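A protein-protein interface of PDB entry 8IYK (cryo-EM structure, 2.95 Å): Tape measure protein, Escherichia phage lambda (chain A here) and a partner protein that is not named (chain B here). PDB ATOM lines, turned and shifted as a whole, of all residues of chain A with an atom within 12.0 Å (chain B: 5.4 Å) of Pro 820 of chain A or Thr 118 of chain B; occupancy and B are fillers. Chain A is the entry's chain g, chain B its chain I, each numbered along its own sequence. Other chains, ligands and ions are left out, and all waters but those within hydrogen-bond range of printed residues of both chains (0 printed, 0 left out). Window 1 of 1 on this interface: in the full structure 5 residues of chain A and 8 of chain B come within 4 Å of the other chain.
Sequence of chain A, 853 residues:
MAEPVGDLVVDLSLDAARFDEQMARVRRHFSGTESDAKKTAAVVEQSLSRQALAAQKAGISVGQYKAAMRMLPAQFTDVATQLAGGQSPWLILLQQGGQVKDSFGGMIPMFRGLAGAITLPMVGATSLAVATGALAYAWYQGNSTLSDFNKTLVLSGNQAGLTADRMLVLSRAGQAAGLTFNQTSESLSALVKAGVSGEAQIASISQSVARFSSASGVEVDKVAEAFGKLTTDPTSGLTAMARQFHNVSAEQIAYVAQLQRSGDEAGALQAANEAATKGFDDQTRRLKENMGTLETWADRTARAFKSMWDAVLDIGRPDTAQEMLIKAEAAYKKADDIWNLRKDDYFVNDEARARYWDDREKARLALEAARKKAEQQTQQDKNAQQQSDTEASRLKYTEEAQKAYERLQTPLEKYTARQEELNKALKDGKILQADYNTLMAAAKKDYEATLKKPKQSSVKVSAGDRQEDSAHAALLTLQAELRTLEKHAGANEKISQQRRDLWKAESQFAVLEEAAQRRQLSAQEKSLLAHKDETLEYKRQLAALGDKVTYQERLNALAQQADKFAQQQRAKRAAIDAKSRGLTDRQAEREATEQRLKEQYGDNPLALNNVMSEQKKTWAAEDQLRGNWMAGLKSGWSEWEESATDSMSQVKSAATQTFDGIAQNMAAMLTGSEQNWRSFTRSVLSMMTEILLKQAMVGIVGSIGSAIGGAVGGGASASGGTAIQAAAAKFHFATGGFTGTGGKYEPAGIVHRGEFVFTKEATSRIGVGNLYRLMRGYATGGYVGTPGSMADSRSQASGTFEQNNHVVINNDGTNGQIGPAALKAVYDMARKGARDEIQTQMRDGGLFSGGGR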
ATOM      1  N   GLN A 817      -6.334 -25.024 -21.226  1.00  0.00           N
ATOM      2  CA  GLN A 817      -5.038 -24.465 -21.592  1.00  0.00           C
ATOM      3  C   GLN A 817      -5.047 -22.945 -21.477  1.00  0.00           C
ATOM      4  O   GLN A 817      -5.870 -22.273 -22.097  1.00  0.00           O
ATOM      5  CB  GLN A 817      -4.658 -24.877 -23.016  1.00  0.00           C
ATOM      6  CG  GLN A 817      -5.821 -24.864 -23.996  1.00  0.00           C
ATOM      7  CD  GLN A 817      -5.868 -23.595 -24.822  1.00  0.00           C
ATOM      8  OE1 GLN A 817      -4.834 -23.061 -25.221  1.00  0.00           O
ATOM      9  NE2 GLN A 817      -7.073 -23.098 -25.076  1.00  0.00           N
ATOM     10  N   ILE A 818      -4.135 -22.404 -20.677  1.00  0.00           N
ATOM     11  CA  ILE A 818      -4.011 -20.957 -20.546  1.00  0.00           C
ATOM     12  C   ILE A 818      -3.265 -20.414 -21.757  1.00  0.00           C
ATOM     13  O   ILE A 818      -2.222 -20.947 -22.155  1.00  0.00           O
ATOM     14  CB  ILE A 818      -3.311 -20.577 -19.231  1.00  0.00           C
ATOM     15  CG1 ILE A 818      -1.986 -21.326 -19.079  1.00  0.00           C
ATOM     16  CG2 ILE A 818      -4.222 -20.857 -18.045  1.00  0.00           C
ATOM     17  CD1 ILE A 818      -1.232 -20.982 -17.810  1.00  0.00           C
ATOM     18  N   GLY A 819      -3.813 -19.361 -22.356  1.00  0.00           N
ATOM     19  CA  GLY A 819      -3.266 -18.770 -23.556  1.00  0.00           C
ATOM     20  C   GLY A 819      -1.825 -18.295 -23.472  1.00  0.00           C
ATOM     21  O   GLY A 819      -1.030 -18.544 -24.385  1.00  0.00           O
ATOM     22  N   PRO A 820      -1.459 -17.573 -22.401  1.00  0.00           N
ATOM     23  CA  PRO A 820      -0.085 -17.043 -22.334  1.00  0.00           C
ATOM     24  C   PRO A 820       0.995 -18.105 -22.453  1.00  0.00           C
ATOM     25  O   PRO A 820       2.000 -17.884 -23.139  1.00  0.00           O
ATOM     26  CB  PRO A 820      -0.042 -16.359 -20.963  1.00  0.00           C
ATOM     27  CG  PRO A 820      -1.434 -16.015 -20.658  1.00  0.00           C
ATOM     28  CD  PRO A 820      -2.308 -17.030 -21.323  1.00  0.00           C
ATOM     29  N   ALA A 821       0.818 -19.255 -21.805  1.00  0.00           N
ATOM     30  CA  ALA A 821       1.819 -20.311 -21.899  1.00  0.00           C
ATOM     31  C   ALA A 821       1.733 -21.061 -23.220  1.00  0.00           C
ATOM     32  O   ALA A 821       2.760 -21.519 -23.734  1.00  0.00           O
ATOM     33  CB  ALA A 821       1.670 -21.284 -20.729  1.00  0.00           C
ATOM     34  N   ALA A 822       0.530 -21.198 -23.779  1.00  0.00           N
ATOM     35  CA  ALA A 822       0.372 -21.950 -25.018  1.00  0.00           C
ATOM     36  C   ALA A 822       0.902 -21.181 -26.220  1.00  0.00           C
ATOM     37  O   ALA A 822       1.329 -21.796 -27.204  1.00  0.00           O
ATOM     38  CB  ALA A 822      -1.098 -22.313 -25.229  1.00  0.00           C
ATOM     39  N   LEU A 823       0.870 -19.848 -26.168  1.00  0.00           N
ATOM     40  CA  LEU A 823       1.335 -19.060 -27.307  1.00  0.00           C
ATOM     41  C   LEU A 823       2.829 -19.251 -27.545  1.00  0.00           C
ATOM     42  O   LEU A 823       3.270 -19.339 -28.696  1.00  0.00           O
ATOM     43  CB  LEU A 823       1.002 -17.584 -27.097  1.00  0.00           C
ATOM     44  CG  LEU A 823      -0.434 -17.177 -27.433  1.00  0.00           C
ATOM     45  CD1 LEU A 823      -0.514 -15.692 -27.738  1.00  0.00           C
ATOM     46  CD2 LEU A 823      -0.977 -17.993 -28.598  1.00  0.00           C
ATOM     47  N   LYS A 824       3.624 -19.318 -26.475  1.00  0.00           N
ATOM     48  CA  LYS A 824       5.053 -19.573 -26.635  1.00  0.00           C
ATOM     49  C   LYS A 824       5.307 -20.944 -27.247  1.00  0.00           C
ATOM     50  O   LYS A 824       6.174 -21.095 -28.118  1.00  0.00           O
ATOM     51  CB  LYS A 824       5.761 -19.453 -25.288  1.00  0.00           C
ATOM     52  CG  LYS A 824       7.277 -19.413 -25.382  1.00  0.00           C
ATOM     53  CD  LYS A 824       7.752 -18.426 -26.430  1.00  0.00           C
ATOM     54  CE  LYS A 824       9.264 -18.471 -26.570  1.00  0.00           C
ATOM     55  NZ  LYS A 824       9.921 -19.008 -25.349  1.00  0.00           N
ATOM     56  N   ALA A 825       4.567 -21.959 -26.798  1.00  0.00           N
ATOM     57  CA  ALA A 825       4.726 -23.293 -27.364  1.00  0.00           C
ATOM     58  C   ALA A 825       4.360 -23.308 -28.842  1.00  0.00           C
ATOM     59  O   ALA A 825       5.052 -23.931 -29.655  1.00  0.00           O
ATOM     60  CB  ALA A 825       3.875 -24.298 -26.589  1.00  0.00           C
ATOM     61  N   VAL A 826       3.274 -22.622 -29.208  1.00  0.00           N
ATOM     62  CA  VAL A 826       2.871 -22.570 -30.611  1.00  0.00           C
ATOM     63  C   VAL A 826       3.927 -21.851 -31.440  1.00  0.00           C
ATOM     64  O   VAL A 826       4.263 -22.280 -32.549  1.00  0.00           O
ATOM     65  CB  VAL A 826       1.487 -21.911 -30.749  1.00  0.00           C
ATOM     66  CG1 VAL A 826       1.143 -21.704 -32.212  1.00  0.00           C
ATOM     67  CG2 VAL A 826       0.427 -22.766 -30.080  1.00  0.00           C
ATOM     68  N   TYR A 827       4.476 -20.754 -30.913  1.00  0.00           N
ATOM     69  CA  TYR A 827       5.516 -20.020 -31.629  1.00  0.00           C
ATOM     70  C   TYR A 827       6.756 -20.878 -31.844  1.00  0.00           C
ATOM     71  O   TYR A 827       7.347 -20.870 -32.930  1.00  0.00           O
ATOM     72  CB  TYR A 827       5.873 -18.750 -30.861  1.00  0.00           C
ATOM     73  CG  TYR A 827       6.876 -17.863 -31.558  1.00  0.00           C
ATOM     74  CD1 TYR A 827       6.516 -17.109 -32.664  1.00  0.00           C
ATOM     75  CD2 TYR A 827       8.182 -17.776 -31.102  1.00  0.00           C
ATOM     76  CE1 TYR A 827       7.433 -16.296 -33.299  1.00  0.00           C
ATOM     77  CE2 TYR A 827       9.105 -16.967 -31.730  1.00  0.00           C
ATOM     78  CZ  TYR A 827       8.725 -16.230 -32.827  1.00  0.00           C
ATOM     79  OH  TYR A 827       9.644 -15.422 -33.455  1.00  0.00           O
ATOM     80  N   ASP A 828       7.167 -21.626 -30.821  1.00  0.00           N
ATOM     81  CA  ASP A 828       8.377 -22.432 -30.952  1.00  0.00           C
ATOM     82  C   ASP A 828       8.155 -23.625 -31.876  1.00  0.00           C
ATOM     83  O   ASP A 828       9.054 -24.004 -32.639  1.00  0.00           O
ATOM     84  CB  ASP A 828       8.847 -22.884 -29.576  1.00  0.00           C
ATOM     85  CG  ASP A 828       9.395 -21.738 -28.747  1.00  0.00           C
ATOM     86  OD1 ASP A 828       8.904 -20.603 -28.913  1.00  0.00           O
ATOM     87  OD2 ASP A 828      10.316 -21.962 -27.936  1.00  0.00           O
ATOM     88  N   MET A 829       6.966 -24.228 -31.829  1.00  0.00           N
ATOM     89  CA  MET A 829       6.642 -25.279 -32.787  1.00  0.00           C
ATOM     90  C   MET A 829       6.613 -24.728 -34.205  1.00  0.00           C
ATOM     91  O   MET A 829       7.026 -25.407 -35.151  1.00  0.00           O
ATOM     92  CB  MET A 829       5.303 -25.923 -32.429  1.00  0.00           C
ATOM     93  CG  MET A 829       4.870 -27.023 -33.380  1.00  0.00           C
ATOM     94  SD  MET A 829       5.591 -28.627 -32.995  1.00  0.00           S
ATOM     95  CE  MET A 829       4.646 -29.080 -31.547  1.00  0.00           C
ATOM     96  N   LEU B 107       0.434  -8.822 -29.989  1.00  0.00           N
ATOM     97  CA  LEU B 107       1.708  -9.330 -29.497  1.00  0.00           C
ATOM     98  C   LEU B 107       2.860  -8.467 -29.997  1.00  0.00           C
ATOM     99  O   LEU B 107       2.847  -7.978 -31.129  1.00  0.00           O
ATOM    100  CB  LEU B 107       1.905 -10.779 -29.933  1.00  0.00           C
ATOM    101  CG  LEU B 107       0.938 -11.789 -29.315  1.00  0.00           C
ATOM    102  CD1 LEU B 107       1.262 -13.197 -29.778  1.00  0.00           C
ATOM    103  CD2 LEU B 107       0.972 -11.701 -27.800  1.00  0.00           C
ATOM    104  N   ALA B 111       6.822 -10.743 -25.652  1.00  0.00           N
ATOM    105  CA  ALA B 111       5.945 -11.903 -25.556  1.00  0.00           C
ATOM    106  C   ALA B 111       6.497 -13.081 -26.350  1.00  0.00           C
ATOM    107  O   ALA B 111       6.503 -14.220 -25.868  1.00  0.00           O
ATOM    108  CB  ALA B 111       4.544 -11.533 -26.040  1.00  0.00           C
ATOM    109  N   ILE B 112       6.959 -12.827 -27.576  1.00  0.00           N
ATOM    110  CA  ILE B 112       7.453 -13.913 -28.415  1.00  0.00           C
ATOM    111  C   ILE B 112       8.798 -14.424 -27.917  1.00  0.00           C
ATOM    112  O   ILE B 112       9.109 -15.612 -28.064  1.00  0.00           O
ATOM    113  CB  ILE B 112       7.521 -13.466 -29.888  1.00  0.00           C
ATOM    114  CG1 ILE B 112       8.514 -12.318 -30.068  1.00  0.00           C
ATOM    115  CG2 ILE B 112       6.141 -13.064 -30.386  1.00  0.00           C
ATOM    116  CD1 ILE B 112       8.607 -11.810 -31.489  1.00  0.00           C
ATOM    117  N   GLY B 114      10.267 -15.608 -25.169  1.00  0.00           N
ATOM    118  CA  GLY B 114       9.946 -16.111 -23.849  1.00  0.00           C
ATOM    119  C   GLY B 114       8.560 -15.689 -23.413  1.00  0.00           C
ATOM    120  O   GLY B 114       8.180 -14.528 -23.587  1.00  0.00           O
ATOM    121  N   SER B 115       7.790 -16.615 -22.842  1.00  0.00           N
ATOM    122  CA  SER B 115       6.439 -16.288 -22.403  1.00  0.00           C
ATOM    123  C   SER B 115       6.483 -15.594 -21.049  1.00  0.00           C
ATOM    124  O   SER B 115       5.809 -16.013 -20.102  1.00  0.00           O
ATOM    125  CB  SER B 115       5.570 -17.545 -22.328  1.00  0.00           C
ATOM    126  OG  SER B 115       5.735 -18.206 -21.087  1.00  0.00           O
ATOM    127  N   PHE B 116       7.277 -14.532 -20.956  1.00  0.00           N
ATOM    128  CA  PHE B 116       7.396 -13.759 -19.730  1.00  0.00           C
ATOM    129  C   PHE B 116       6.304 -12.711 -19.598  1.00  0.00           C
ATOM    130  O   PHE B 116       5.880 -12.404 -18.477  1.00  0.00           O
ATOM    131  CB  PHE B 116       8.762 -13.074 -19.671  1.00  0.00           C
ATOM    132  CG  PHE B 116       9.903 -13.958 -20.084  1.00  0.00           C
ATOM    133  CD1 PHE B 116       9.982 -15.267 -19.638  1.00  0.00           C
ATOM    134  CD2 PHE B 116      10.894 -13.479 -20.923  1.00  0.00           C
ATOM    135  CE1 PHE B 116      11.029 -16.080 -20.019  1.00  0.00           C
ATOM    136  CE2 PHE B 116      11.944 -14.288 -21.307  1.00  0.00           C
ATOM    137  CZ  PHE B 116      12.011 -15.590 -20.854  1.00  0.00           C
ATOM    138  N   PHE B 117       5.842 -12.157 -20.718  1.00  0.00           N
ATOM    139  CA  PHE B 117       4.852 -11.096 -20.701  1.00  0.00           C
ATOM    140  C   PHE B 117       3.600 -11.418 -21.501  1.00  0.00           C
ATOM    141  O   PHE B 117       2.717 -10.560 -21.610  1.00  0.00           O
ATOM    142  CB  PHE B 117       5.478  -9.787 -21.196  1.00  0.00           C
ATOM    143  CG  PHE B 117       5.736  -8.805 -20.096  1.00  0.00           C
ATOM    144  CD1 PHE B 117       4.684  -8.297 -19.353  1.00  0.00           C
ATOM    145  CD2 PHE B 117       7.025  -8.445 -19.756  1.00  0.00           C
ATOM    146  CE1 PHE B 117       4.911  -7.410 -18.327  1.00  0.00           C
ATOM    147  CE2 PHE B 117       7.256  -7.568 -18.721  1.00  0.00           C
ATOM    148  CZ  PHE B 117       6.197  -7.045 -18.011  1.00  0.00           C
ATOM    149  N   THR B 118       3.497 -12.622 -22.066  1.00  0.00           N
ATOM    150  CA  THR B 118       2.188 -13.112 -22.480  1.00  0.00           C
ATOM    151  C   THR B 118       1.272 -13.239 -21.272  1.00  0.00           C
ATOM    152  O   THR B 118       0.078 -12.927 -21.346  1.00  0.00           O
ATOM    153  CB  THR B 118       2.321 -14.456 -23.195  1.00  0.00           C
ATOM    154  OG1 THR B 118       3.334 -15.241 -22.554  1.00  0.00           O
ATOM    155  CG2 THR B 118       2.685 -14.257 -24.656  1.00  0.00           C
ATOM    156  N   ALA B 119       1.821 -13.699 -20.147  1.00  0.00           N
ATOM    157  CA  ALA B 119       1.117 -13.690 -18.874  1.00  0.00           C
ATOM    158  C   ALA B 119       1.183 -12.339 -18.177  1.00  0.00           C
ATOM    159  O   ALA B 119       0.530 -12.163 -17.144  1.00  0.00           O
ATOM    160  CB  ALA B 119       1.683 -14.773 -17.951  1.00  0.00           C
ATOM    161  N   GLY B 120       1.965 -11.392 -18.703  1.00  0.00           N
ATOM    162  CA  GLY B 120       1.931 -10.042 -18.164  1.00  0.00           C
ATOM    163  C   GLY B 120       0.581  -9.383 -18.362  1.00  0.00           C
ATOM    164  O   GLY B 120       0.056  -8.729 -17.459  1.00  0.00           O
ATOM    165  N   ALA B 121       0.002  -9.546 -19.551  1.00  0.00           N
ATOM    166  CA  ALA B 121      -1.387  -9.182 -19.788  1.00  0.00           C
ATOM    167  C   ALA B 121      -2.350 -10.283 -19.368  1.00  0.00           C
ATOM    168  O   ALA B 121      -3.563 -10.048 -19.341  1.00  0.00           O
ATOM    169  CB  ALA B 121      -1.593  -8.847 -21.266  1.00  0.00           C
ATOM    170  N   THR B 122      -1.827 -11.478 -19.081  1.00  0.00           N
ATOM    171  CA  THR B 122      -2.534 -12.639 -18.540  1.00  0.00           C
ATOM    172  C   THR B 122      -3.463 -13.289 -19.559  1.00  0.00           C
ATOM    173  O   THR B 122      -3.928 -14.411 -19.331  1.00  0.00           O
ATOM    174  CB  THR B 122      -3.334 -12.272 -17.280  1.00  0.00           C
ATOM    175  OG1 THR B 122      -4.452 -11.448 -17.636  1.00  0.00           O
ATOM    176  CG2 THR B 122      -2.461 -11.541 -16.268  1.00  0.00           C
ATOM    177  N   LEU B 123      -3.711 -12.611 -20.686  1.00  0.00           N
ATOM    178  CA  LEU B 123      -4.489 -13.132 -21.810  1.00  0.00           C
ATOM    179  C   LEU B 123      -5.710 -13.903 -21.311  1.00  0.00           C
ATOM    180  O   LEU B 123      -6.058 -14.959 -21.846  1.00  0.00           O
ATOM    181  CB  LEU B 123      -3.581 -13.993 -22.701  1.00  0.00           C
ATOM    182  CG  LEU B 123      -3.838 -14.264 -24.190  1.00  0.00           C
ATOM    183  CD1 LEU B 123      -2.506 -14.545 -24.859  1.00  0.00           C
ATOM    184  CD2 LEU B 123      -4.767 -15.436 -24.446  1.00  0.00           C
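Of chain B, only Ser 115, Thr 118, Ala 119, Thr 122 and Leu 123 come within 4 Å of Pro 820 of chain A. Ala 821 of chain A touches none of the printed residues of chain B. Printed residues of chain B within 4 Å of Leu 823 of chain A: Leu 107 (3.7 Å) and Leu 123 (3.7 Å). Ala 825 of chain A touches none of the printed residues of chain B. Of the printed residues of chain B, Tyr 827 of chain A touches Ile 112 (3.8 Å). No residue of chain A comes within 4 Å of Ala 111 of chain B. Thr 118 of chain B touches one residue of chain A. Of chain A, only Pro 820 comes within 4 Å of Ala 119 of chain B. No residue of chain A comes within 4 Å of Gly 120 of chain B. Ala 121 of chain B touches none of the printed residues of chain A. Thr 122 of chain B touches just one residue of chain A: Pro 820. Of chain A, only Gly 819 (3.8 Å), Pro 820 (3.6 Å) and Leu 823 (3.7 Å) come within 4 Å of Leu 123 of chain B. The nearest printed residue of chain B that does not touch Pro 820 of chain A is Gly 120 of chain B (5.8 Å).
The backbone carbonyl oxygen (O) of Pro 820 of chain A is in hydrogen-bond range of the side-chain hydroxyl (OG1) of Thr 118 of chain B (3.0 Å). N of Gly 114 of chain B sits close to NZ of Lys 824 of chain A (3.4 Å).
Hydrophobic or aromatic side chains of chain A that line the printed part of chain B: Pro 820, Leu 823 and Tyr 827. Of the 13 printed residues of chain B, 8 touch a printed residue of chain A. Printed residues of chain B that touch a printed residue of chain A: Leu 107, Ile 112, Gly 114, Ser 115, Thr 118, Ala 119, Thr 122 and Leu 123. Hydrophobic or aromatic side chains of chain B that line the printed part of chain A: Leu 107, Ala 119 and Leu 123. Among the printed residues, 12 pairs touch across the chains.
Among the printed residues, merely in contact across the chains: Lys 824 of chain A with Ile 112 of chain B, Pro 820 of chain A with Thr 122 of chain B, Pro 820 of chain A with Ala 119 of chain B, Lys 824 of chain A with Ser 115 of chain B, Pro 820 of chain A with Leu 123 of chain B, Pro 820 of chain A with Ser 115 of chain B, Leu 823 of chain A with Leu 107 of chain B, Leu 823 of chain A with Leu 123 of chain B, Gly 819 of chain A with Leu 123 of chain B and Tyr 827 of chain A with Ile 112 of chain B.
NZ of Lys 824 of chain A lies within salt-bridge range of OD2 of Asp 828 of chain A (3.9 Å).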
